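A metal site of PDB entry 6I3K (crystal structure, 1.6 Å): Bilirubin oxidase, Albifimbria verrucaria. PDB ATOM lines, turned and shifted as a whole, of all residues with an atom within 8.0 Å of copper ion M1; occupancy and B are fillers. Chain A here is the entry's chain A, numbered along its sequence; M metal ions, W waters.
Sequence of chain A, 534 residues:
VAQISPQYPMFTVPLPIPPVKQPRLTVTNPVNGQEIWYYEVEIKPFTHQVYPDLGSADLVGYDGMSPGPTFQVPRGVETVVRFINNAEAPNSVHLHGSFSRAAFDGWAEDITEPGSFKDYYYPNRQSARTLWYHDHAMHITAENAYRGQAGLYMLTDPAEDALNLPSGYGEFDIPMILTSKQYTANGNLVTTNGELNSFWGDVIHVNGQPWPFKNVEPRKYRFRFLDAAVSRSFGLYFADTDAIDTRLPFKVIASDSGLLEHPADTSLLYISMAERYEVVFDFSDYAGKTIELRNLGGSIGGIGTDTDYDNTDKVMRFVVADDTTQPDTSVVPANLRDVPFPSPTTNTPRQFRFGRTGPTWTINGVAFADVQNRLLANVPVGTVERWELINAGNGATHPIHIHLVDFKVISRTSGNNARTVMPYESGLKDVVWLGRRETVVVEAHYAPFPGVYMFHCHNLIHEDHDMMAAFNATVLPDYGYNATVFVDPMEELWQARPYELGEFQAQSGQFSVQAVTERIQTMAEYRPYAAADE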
ATOM      1  N   HIS A  94      -9.447 -17.183  27.806  1.00  0.00           N
ATOM      2  CA  HIS A  94     -10.469 -16.618  26.902  1.00  0.00           C
ATOM      3  C   HIS A  94     -10.049 -15.239  26.396  1.00  0.00           C
ATOM      4  O   HIS A  94      -9.768 -14.364  27.256  1.00  0.00           O
ATOM      5  CB  HIS A  94     -11.815 -16.479  27.606  1.00  0.00           C
ATOM      6  CG  HIS A  94     -12.866 -15.780  26.827  1.00  0.00           C
ATOM      7  ND1 HIS A  94     -13.169 -16.082  25.499  1.00  0.00           N
ATOM      8  CD2 HIS A  94     -13.668 -14.768  27.187  1.00  0.00           C
ATOM      9  CE1 HIS A  94     -14.145 -15.294  25.099  1.00  0.00           C
ATOM     10  NE2 HIS A  94     -14.448 -14.483  26.095  1.00  0.00           N
ATOM     11  N   HIS A  96     -11.551 -12.270  25.267  1.00  0.00           N
ATOM     12  CA  HIS A  96     -12.907 -11.684  25.347  1.00  0.00           C
ATOM     13  C   HIS A  96     -13.031 -10.550  24.303  1.00  0.00           C
ATOM     14  O   HIS A  96     -12.236  -9.579  24.352  1.00  0.00           O
ATOM     15  CB  HIS A  96     -13.143 -11.212  26.788  1.00  0.00           C
ATOM     16  CG  HIS A  96     -14.512 -10.678  27.040  1.00  0.00           C
ATOM     17  ND1 HIS A  96     -15.208 -10.966  28.198  1.00  0.00           N
ATOM     18  CD2 HIS A  96     -15.308  -9.873  26.309  1.00  0.00           C
ATOM     19  CE1 HIS A  96     -16.389 -10.376  28.143  1.00  0.00           C
ATOM     20  NE2 HIS A  96     -16.490  -9.695  27.000  1.00  0.00           N
ATOM     21  N   ASP A 105     -11.363 -20.586  22.277  1.00  0.00           N
ATOM     22  CA  ASP A 105     -12.207 -19.529  22.899  1.00  0.00           C
ATOM     23  C   ASP A 105     -12.131 -19.568  24.431  1.00  0.00           C
ATOM     24  O   ASP A 105     -12.757 -18.640  25.038  1.00  0.00           O
ATOM     25  CB  ASP A 105     -13.662 -19.648  22.427  1.00  0.00           C
ATOM     26  CG  ASP A 105     -14.534 -18.416  22.711  1.00  0.00           C
ATOM     27  OD1 ASP A 105     -14.031 -17.303  22.421  1.00  0.00           O
ATOM     28  OD2 ASP A 105     -15.697 -18.590  23.211  1.00  0.00           O
ATOM     29  N   GLY A 106     -11.520 -20.562  25.080  1.00  0.00           N
ATOM     30  CA  GLY A 106     -11.490 -20.571  26.562  1.00  0.00           C
ATOM     31  C   GLY A 106     -12.720 -21.219  27.163  1.00  0.00           C
ATOM     32  O   GLY A 106     -13.120 -20.876  28.293  1.00  0.00           O
ATOM     33  N   TRP A 107     -13.311 -22.196  26.471  1.00  0.00           N
ATOM     34  CA  TRP A 107     -14.361 -23.072  27.060  1.00  0.00           C
ATOM     35  C   TRP A 107     -13.909 -23.505  28.462  1.00  0.00           C
ATOM     36  O   TRP A 107     -12.708 -23.879  28.636  1.00  0.00           O
ATOM     37  CB  TRP A 107     -14.584 -24.256  26.105  1.00  0.00           C
ATOM     38  CG  TRP A 107     -15.571 -25.271  26.594  1.00  0.00           C
ATOM     39  CD1 TRP A 107     -15.290 -26.472  27.177  1.00  0.00           C
ATOM     40  CD2 TRP A 107     -16.997 -25.180  26.526  1.00  0.00           C
ATOM     41  NE1 TRP A 107     -16.449 -27.128  27.472  1.00  0.00           N
ATOM     42  CE2 TRP A 107     -17.513 -26.365  27.087  1.00  0.00           C
ATOM     43  CE3 TRP A 107     -17.884 -24.197  26.065  1.00  0.00           C
ATOM     44  CZ2 TRP A 107     -18.891 -26.589  27.166  1.00  0.00           C
ATOM     45  CZ3 TRP A 107     -19.237 -24.422  26.118  1.00  0.00           C
ATOM     46  CH2 TRP A 107     -19.741 -25.626  26.657  1.00  0.00           C
ATOM     47  N   ALA A 108     -14.795 -23.410  29.453  1.00  0.00           N
ATOM     48  CA  ALA A 108     -14.382 -23.515  30.877  1.00  0.00           C
ATOM     49  C   ALA A 108     -13.825 -24.915  31.206  1.00  0.00           C
ATOM     50  O   ALA A 108     -13.020 -24.975  32.145  1.00  0.00           O
ATOM     51  CB  ALA A 108     -15.568 -23.164  31.760  1.00  0.00           C
ATOM     52  N   HIS A 134      -8.306 -13.345  29.641  1.00  0.00           N
ATOM     53  CA  HIS A 134      -8.408 -13.666  31.085  1.00  0.00           C
ATOM     54  C   HIS A 134      -8.673 -15.154  31.285  1.00  0.00           C
ATOM     55  O   HIS A 134      -9.134 -15.862  30.369  1.00  0.00           O
ATOM     56  CB  HIS A 134      -9.496 -12.783  31.748  1.00  0.00           C
ATOM     57  CG  HIS A 134     -10.881 -13.036  31.276  1.00  0.00           C
ATOM     58  ND1 HIS A 134     -11.668 -14.074  31.766  1.00  0.00           N
ATOM     59  CD2 HIS A 134     -11.692 -12.334  30.444  1.00  0.00           C
ATOM     60  CE1 HIS A 134     -12.859 -14.022  31.185  1.00  0.00           C
ATOM     61  NE2 HIS A 134     -12.922 -12.915  30.437  1.00  0.00           N
ATOM     62  N   ASP A 135      -8.478 -15.592  32.531  1.00  0.00           N
ATOM     63  CA  ASP A 135      -8.742 -17.011  32.830  1.00  0.00           C
ATOM     64  C   ASP A 135     -10.223 -17.283  32.795  1.00  0.00           C
ATOM     65  O   ASP A 135     -11.064 -16.387  33.116  1.00  0.00           O
ATOM     66  CB  ASP A 135      -8.183 -17.444  34.190  1.00  0.00           C
ATOM     67  CG  ASP A 135      -8.234 -18.967  34.271  1.00  0.00           C
ATOM     68  OD1 ASP A 135      -7.498 -19.581  33.461  1.00  0.00           O
ATOM     69  OD2 ASP A 135      -9.006 -19.492  35.073  1.00  0.00           O
ATOM     70  N   HIS A 136     -10.589 -18.517  32.465  1.00  0.00           N
ATOM     71  CA  HIS A 136     -11.978 -18.977  32.363  1.00  0.00           C
ATOM     72  C   HIS A 136     -12.150 -20.416  32.874  1.00  0.00           C
ATOM     73  O   HIS A 136     -13.192 -21.016  32.524  1.00  0.00           O
ATOM     74  CB  HIS A 136     -12.440 -18.850  30.894  1.00  0.00           C
ATOM     75  CG  HIS A 136     -13.841 -18.394  30.731  1.00  0.00           C
ATOM     76  ND1 HIS A 136     -14.938 -19.048  31.310  1.00  0.00           N
ATOM     77  CD2 HIS A 136     -14.353 -17.344  30.027  1.00  0.00           C
ATOM     78  CE1 HIS A 136     -16.051 -18.363  31.007  1.00  0.00           C
ATOM     79  NE2 HIS A 136     -15.749 -17.305  30.205  1.00  0.00           N
ATOM     80  N   THR A 141     -12.442 -19.543  38.139  1.00  0.00           N
ATOM     81  CA  THR A 141     -12.250 -18.319  37.310  1.00  0.00           C
ATOM     82  C   THR A 141     -12.075 -17.105  38.231  1.00  0.00           C
ATOM     83  O   THR A 141     -11.174 -16.265  37.977  1.00  0.00           O
ATOM     84  CB  THR A 141     -13.410 -18.142  36.327  1.00  0.00           C
ATOM     85  OG1 THR A 141     -13.333 -19.181  35.355  1.00  0.00           O
ATOM     86  CG2 THR A 141     -13.346 -16.806  35.603  1.00  0.00           C
ATOM     87  N   ALA A 274     -16.464  -6.821  32.919  1.00  0.00           N
ATOM     88  CA  ALA A 274     -16.062  -7.271  31.563  1.00  0.00           C
ATOM     89  C   ALA A 274     -16.396  -6.229  30.493  1.00  0.00           C
ATOM     90  O   ALA A 274     -15.989  -6.409  29.330  1.00  0.00           O
ATOM     91  CB  ALA A 274     -16.636  -8.648  31.207  1.00  0.00           C
ATOM     92  N   HIS A 401     -22.823 -11.719  29.468  1.00  0.00           N
ATOM     93  CA  HIS A 401     -21.864 -11.803  28.345  1.00  0.00           C
ATOM     94  C   HIS A 401     -22.242 -12.972  27.452  1.00  0.00           C
ATOM     95  O   HIS A 401     -22.525 -14.082  27.972  1.00  0.00           O
ATOM     96  CB  HIS A 401     -20.431 -11.962  28.878  1.00  0.00           C
ATOM     97  CG  HIS A 401     -19.439 -12.168  27.792  1.00  0.00           C
ATOM     98  ND1 HIS A 401     -19.400 -11.364  26.634  1.00  0.00           N
ATOM     99  CD2 HIS A 401     -18.417 -13.034  27.721  1.00  0.00           C
ATOM    100  CE1 HIS A 401     -18.374 -11.789  25.881  1.00  0.00           C
ATOM    101  NE2 HIS A 401     -17.731 -12.794  26.545  1.00  0.00           N
ATOM    102  N   ILE A 402     -22.282 -12.734  26.133  1.00  0.00           N
ATOM    103  CA  ILE A 402     -22.527 -13.786  25.126  1.00  0.00           C
ATOM    104  C   ILE A 402     -21.227 -13.910  24.330  1.00  0.00           C
ATOM    105  O   ILE A 402     -20.809 -12.910  23.713  1.00  0.00           O
ATOM    106  CB  ILE A 402     -23.750 -13.462  24.271  1.00  0.00           C
ATOM    107  CG1 ILE A 402     -24.983 -13.133  25.121  1.00  0.00           C
ATOM    108  CG2 ILE A 402     -23.989 -14.601  23.287  1.00  0.00           C
ATOM    109  CD1 ILE A 402     -26.156 -12.647  24.306  1.00  0.00           C
ATOM    110  N   HIS A 403     -20.621 -15.097  24.282  1.00  0.00           N
ATOM    111  CA  HIS A 403     -19.424 -15.326  23.453  1.00  0.00           C
ATOM    112  C   HIS A 403     -19.804 -15.286  21.968  1.00  0.00           C
ATOM    113  O   HIS A 403     -20.997 -15.274  21.620  1.00  0.00           O
ATOM    114  CB  HIS A 403     -18.749 -16.660  23.858  1.00  0.00           C
ATOM    115  CG  HIS A 403     -17.973 -16.647  25.142  1.00  0.00           C
ATOM    116  ND1 HIS A 403     -16.715 -17.155  25.222  1.00  0.00           N
ATOM    117  CD2 HIS A 403     -18.301 -16.265  26.395  1.00  0.00           C
ATOM    118  CE1 HIS A 403     -16.262 -17.046  26.465  1.00  0.00           C
ATOM    119  NE2 HIS A 403     -17.217 -16.483  27.213  1.00  0.00           N
ATOM    120  N   TYR A 453     -20.530 -22.527  22.325  1.00  0.00           N
ATOM    121  CA  TYR A 453     -20.010 -21.314  22.982  1.00  0.00           C
ATOM    122  C   TYR A 453     -20.756 -21.060  24.299  1.00  0.00           C
ATOM    123  O   TYR A 453     -21.910 -21.446  24.463  1.00  0.00           O
ATOM    124  CB  TYR A 453     -20.211 -20.089  22.070  1.00  0.00           C
ATOM    125  CG  TYR A 453     -19.295 -20.055  20.862  1.00  0.00           C
ATOM    126  CD1 TYR A 453     -18.001 -19.556  20.980  1.00  0.00           C
ATOM    127  CD2 TYR A 453     -19.746 -20.429  19.601  1.00  0.00           C
ATOM    128  CE1 TYR A 453     -17.146 -19.493  19.877  1.00  0.00           C
ATOM    129  CE2 TYR A 453     -18.901 -20.376  18.497  1.00  0.00           C
ATOM    130  CZ  TYR A 453     -17.610 -19.885  18.637  1.00  0.00           C
ATOM    131  OH  TYR A 453     -16.780 -19.778  17.532  1.00  0.00           O
ATOM    132  N   MET A 454     -20.083 -20.387  25.206  1.00  0.00           N
ATOM    133  CA  MET A 454     -20.647 -20.043  26.535  1.00  0.00           C
ATOM    134  C   MET A 454     -21.421 -18.715  26.475  1.00  0.00           C
ATOM    135  O   MET A 454     -21.134 -17.825  25.642  1.00  0.00           O
ATOM    136  CB  MET A 454     -19.549 -19.941  27.583  1.00  0.00           C
ATOM    137  CG  MET A 454     -18.785 -21.259  27.851  1.00  0.00           C
ATOM    138  SD  MET A 454     -17.431 -21.193  28.963  1.00  0.00           S
ATOM    139  CE  MET A 454     -16.300 -20.078  28.123  1.00  0.00           C
ATOM    140  N   PHE A 455     -22.348 -18.567  27.416  1.00  0.00           N
ATOM    141  CA  PHE A 455     -22.929 -17.240  27.803  1.00  0.00           C
ATOM    142  C   PHE A 455     -23.180 -17.309  29.310  1.00  0.00           C
ATOM    143  O   PHE A 455     -23.414 -18.397  29.846  1.00  0.00           O
ATOM    144  CB  PHE A 455     -24.142 -16.861  26.979  1.00  0.00           C
ATOM    145  CG  PHE A 455     -25.431 -17.608  27.250  1.00  0.00           C
ATOM    146  CD1 PHE A 455     -25.639 -18.896  26.731  1.00  0.00           C
ATOM    147  CD2 PHE A 455     -26.454 -17.028  27.992  1.00  0.00           C
ATOM    148  CE1 PHE A 455     -26.831 -19.572  26.930  1.00  0.00           C
ATOM    149  CE2 PHE A 455     -27.646 -17.711  28.179  1.00  0.00           C
ATOM    150  CZ  PHE A 455     -27.842 -18.960  27.633  1.00  0.00           C
ATOM    151  N   HIS A 456     -23.098 -16.179  29.996  1.00  0.00           N
ATOM    152  CA  HIS A 456     -23.029 -16.207  31.469  1.00  0.00           C
ATOM    153  C   HIS A 456     -23.119 -14.805  32.036  1.00  0.00           C
ATOM    154  O   HIS A 456     -22.842 -13.812  31.347  1.00  0.00           O
ATOM    155  CB  HIS A 456     -21.737 -16.872  31.952  1.00  0.00           C
ATOM    156  CG  HIS A 456     -20.461 -16.267  31.435  1.00  0.00           C
ATOM    157  ND1 HIS A 456     -19.699 -15.438  32.189  1.00  0.00           N
ATOM    158  CD2 HIS A 456     -19.783 -16.442  30.274  1.00  0.00           C
ATOM    159  CE1 HIS A 456     -18.568 -15.174  31.553  1.00  0.00           C
ATOM    160  NE2 HIS A 456     -18.615 -15.730  30.351  1.00  0.00           N
ATOM    161  N   CYS A 457     -23.455 -14.742  33.315  1.00  0.00           N
ATOM    162  CA  CYS A 457     -23.127 -13.567  34.140  1.00  0.00           C
ATOM    163  C   CYS A 457     -21.593 -13.462  34.266  1.00  0.00           C
ATOM    164  O   CYS A 457     -20.941 -14.496  34.530  1.00  0.00           O
ATOM    165  CB  CYS A 457     -23.794 -13.665  35.492  1.00  0.00           C
ATOM    166  SG  CYS A 457     -23.395 -12.265  36.545  1.00  0.00           S
ATOM    167  N   HIS A 458     -21.033 -12.246  34.184  1.00  0.00           N
ATOM    168  CA  HIS A 458     -19.591 -12.006  34.320  1.00  0.00           C
ATOM    169  C   HIS A 458     -19.205 -11.465  35.704  1.00  0.00           C
ATOM    170  O   HIS A 458     -18.019 -11.084  35.891  1.00  0.00           O
ATOM    171  CB  HIS A 458     -19.100 -11.130  33.140  1.00  0.00           C
ATOM    172  CG  HIS A 458     -17.746 -11.498  32.615  1.00  0.00           C
ATOM    173  ND1 HIS A 458     -16.600 -11.434  33.360  1.00  0.00           N
ATOM    174  CD2 HIS A 458     -17.365 -11.871  31.379  1.00  0.00           C
ATOM    175  CE1 HIS A 458     -15.567 -11.797  32.608  1.00  0.00           C
ATOM    176  NE2 HIS A 458     -16.024 -12.032  31.381  1.00  0.00           N
ATOM    177  N   LEU A 460     -17.761 -12.789  38.650  1.00  0.00           N
ATOM    178  CA  LEU A 460     -16.997 -14.063  38.564  1.00  0.00           C
ATOM    179  C   LEU A 460     -17.456 -15.005  39.700  1.00  0.00           C
ATOM    180  O   LEU A 460     -17.382 -16.240  39.510  1.00  0.00           O
ATOM    181  CB  LEU A 460     -15.489 -13.836  38.584  1.00  0.00           C
ATOM    182  CG  LEU A 460     -14.970 -12.869  37.494  1.00  0.00           C
ATOM    183  CD1 LEU A 460     -13.458 -12.771  37.601  1.00  0.00           C
ATOM    184  CD2 LEU A 460     -15.343 -13.282  36.083  1.00  0.00           C
ATOM    185  N   GLU A 463     -20.664 -16.535  38.263  1.00  0.00           N
ATOM    186  CA  GLU A 463     -20.189 -17.401  37.155  1.00  0.00           C
ATOM    187  C   GLU A 463     -19.711 -18.745  37.692  1.00  0.00           C
ATOM    188  O   GLU A 463     -20.087 -19.781  37.119  1.00  0.00           O
ATOM    189  CB  GLU A 463     -19.060 -16.637  36.441  1.00  0.00           C
ATOM    190  CG  GLU A 463     -18.449 -17.391  35.265  1.00  0.00           C
ATOM    191  CD  GLU A 463     -17.455 -16.551  34.474  1.00  0.00           C
ATOM    192  OE1 GLU A 463     -17.581 -15.298  34.485  1.00  0.00           O
ATOM    193  OE2 GLU A 463     -16.520 -17.168  33.874  1.00  0.00           O
ATOM    194  N   MET A 468     -23.842 -19.932  34.316  1.00  0.00           N
ATOM    195  CA  MET A 468     -23.289 -20.007  32.952  1.00  0.00           C
ATOM    196  C   MET A 468     -23.964 -21.165  32.217  1.00  0.00           C
ATOM    197  O   MET A 468     -24.400 -22.132  32.873  1.00  0.00           O
ATOM    198  CB  MET A 468     -21.776 -20.167  33.086  1.00  0.00           C
ATOM    199  CG  MET A 468     -21.054 -20.339  31.767  1.00  0.00           C
ATOM    200  SD  MET A 468     -19.371 -19.800  31.897  1.00  0.00           S
ATOM    201  CE  MET A 468     -18.578 -21.309  32.462  1.00  0.00           C
ATOM    202  N   ALA A 469     -24.134 -21.008  30.903  1.00  0.00           N
ATOM    203  CA  ALA A 469     -24.786 -21.999  30.037  1.00  0.00           C
ATOM    204  C   ALA A 469     -24.106 -21.971  28.680  1.00  0.00           C
ATOM    205  O   ALA A 469     -23.078 -21.269  28.501  1.00  0.00           O
ATOM    206  CB  ALA A 469     -26.256 -21.716  29.919  1.00  0.00           C
HETATM  207 CU    CU M   1     -17.102 -16.324  29.173  1.00  0.00          CU
HETATM  208 CU    CU M   2     -16.102 -13.552  26.050  1.00  0.00          CU
HETATM  209 CU    CU M   3     -14.626 -12.065  29.766  1.00  0.00          CU
HETATM  210  O   HOH W   1     -15.762 -14.365  29.731  1.00  0.00           O
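NE2 of His 136 is bound to copper ion M1 (2.0 Å).
Copper ion M1 is bound by NE2 of His 403 (2.0 Å).
Copper ion M1 is bound by NE2 of His 456, at 2.0 Å.
Copper ion M1 is bound by water W1.
Merely in contact with copper ion M1: His 401 (3.8 Å) and Met 454 (3.98 Å).
Within 4 Å of copper ion M1: His 136, His 401, His 403, Met 454 and His 456.
The nearest printed residue that does not touch copper ion M1 is His 94 (4.3 Å).
The side-chain hydroxyl (OG1) of Thr 141 lies close to the backbone carbonyl oxygen (O) of His 136, at 3.4 Å.
The backbone carbonyl oxygen (O) of Met 454 sits at hydrogen-bond distance from the backbone NH (N) of His 403 (3.1 Å).
ND1 of His 403 lies within hydrogen-bond range of OD2 of Asp 105.
The backbone carbonyl oxygen (O) of His 456 sits at hydrogen-bond distance from the backbone NH (N) of His 401, at 2.8 Å.
ND1 of His 456 lies close to OE1 of Glu 463 (3.1 Å).
A ring nitrogen (NE2) of His 96 sits close to a ring nitrogen (ND1) of His 401, at 3.4 Å.
N of Ala 108 sits at hydrogen-bond distance from SD of Met 454, 3.5 Å away.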
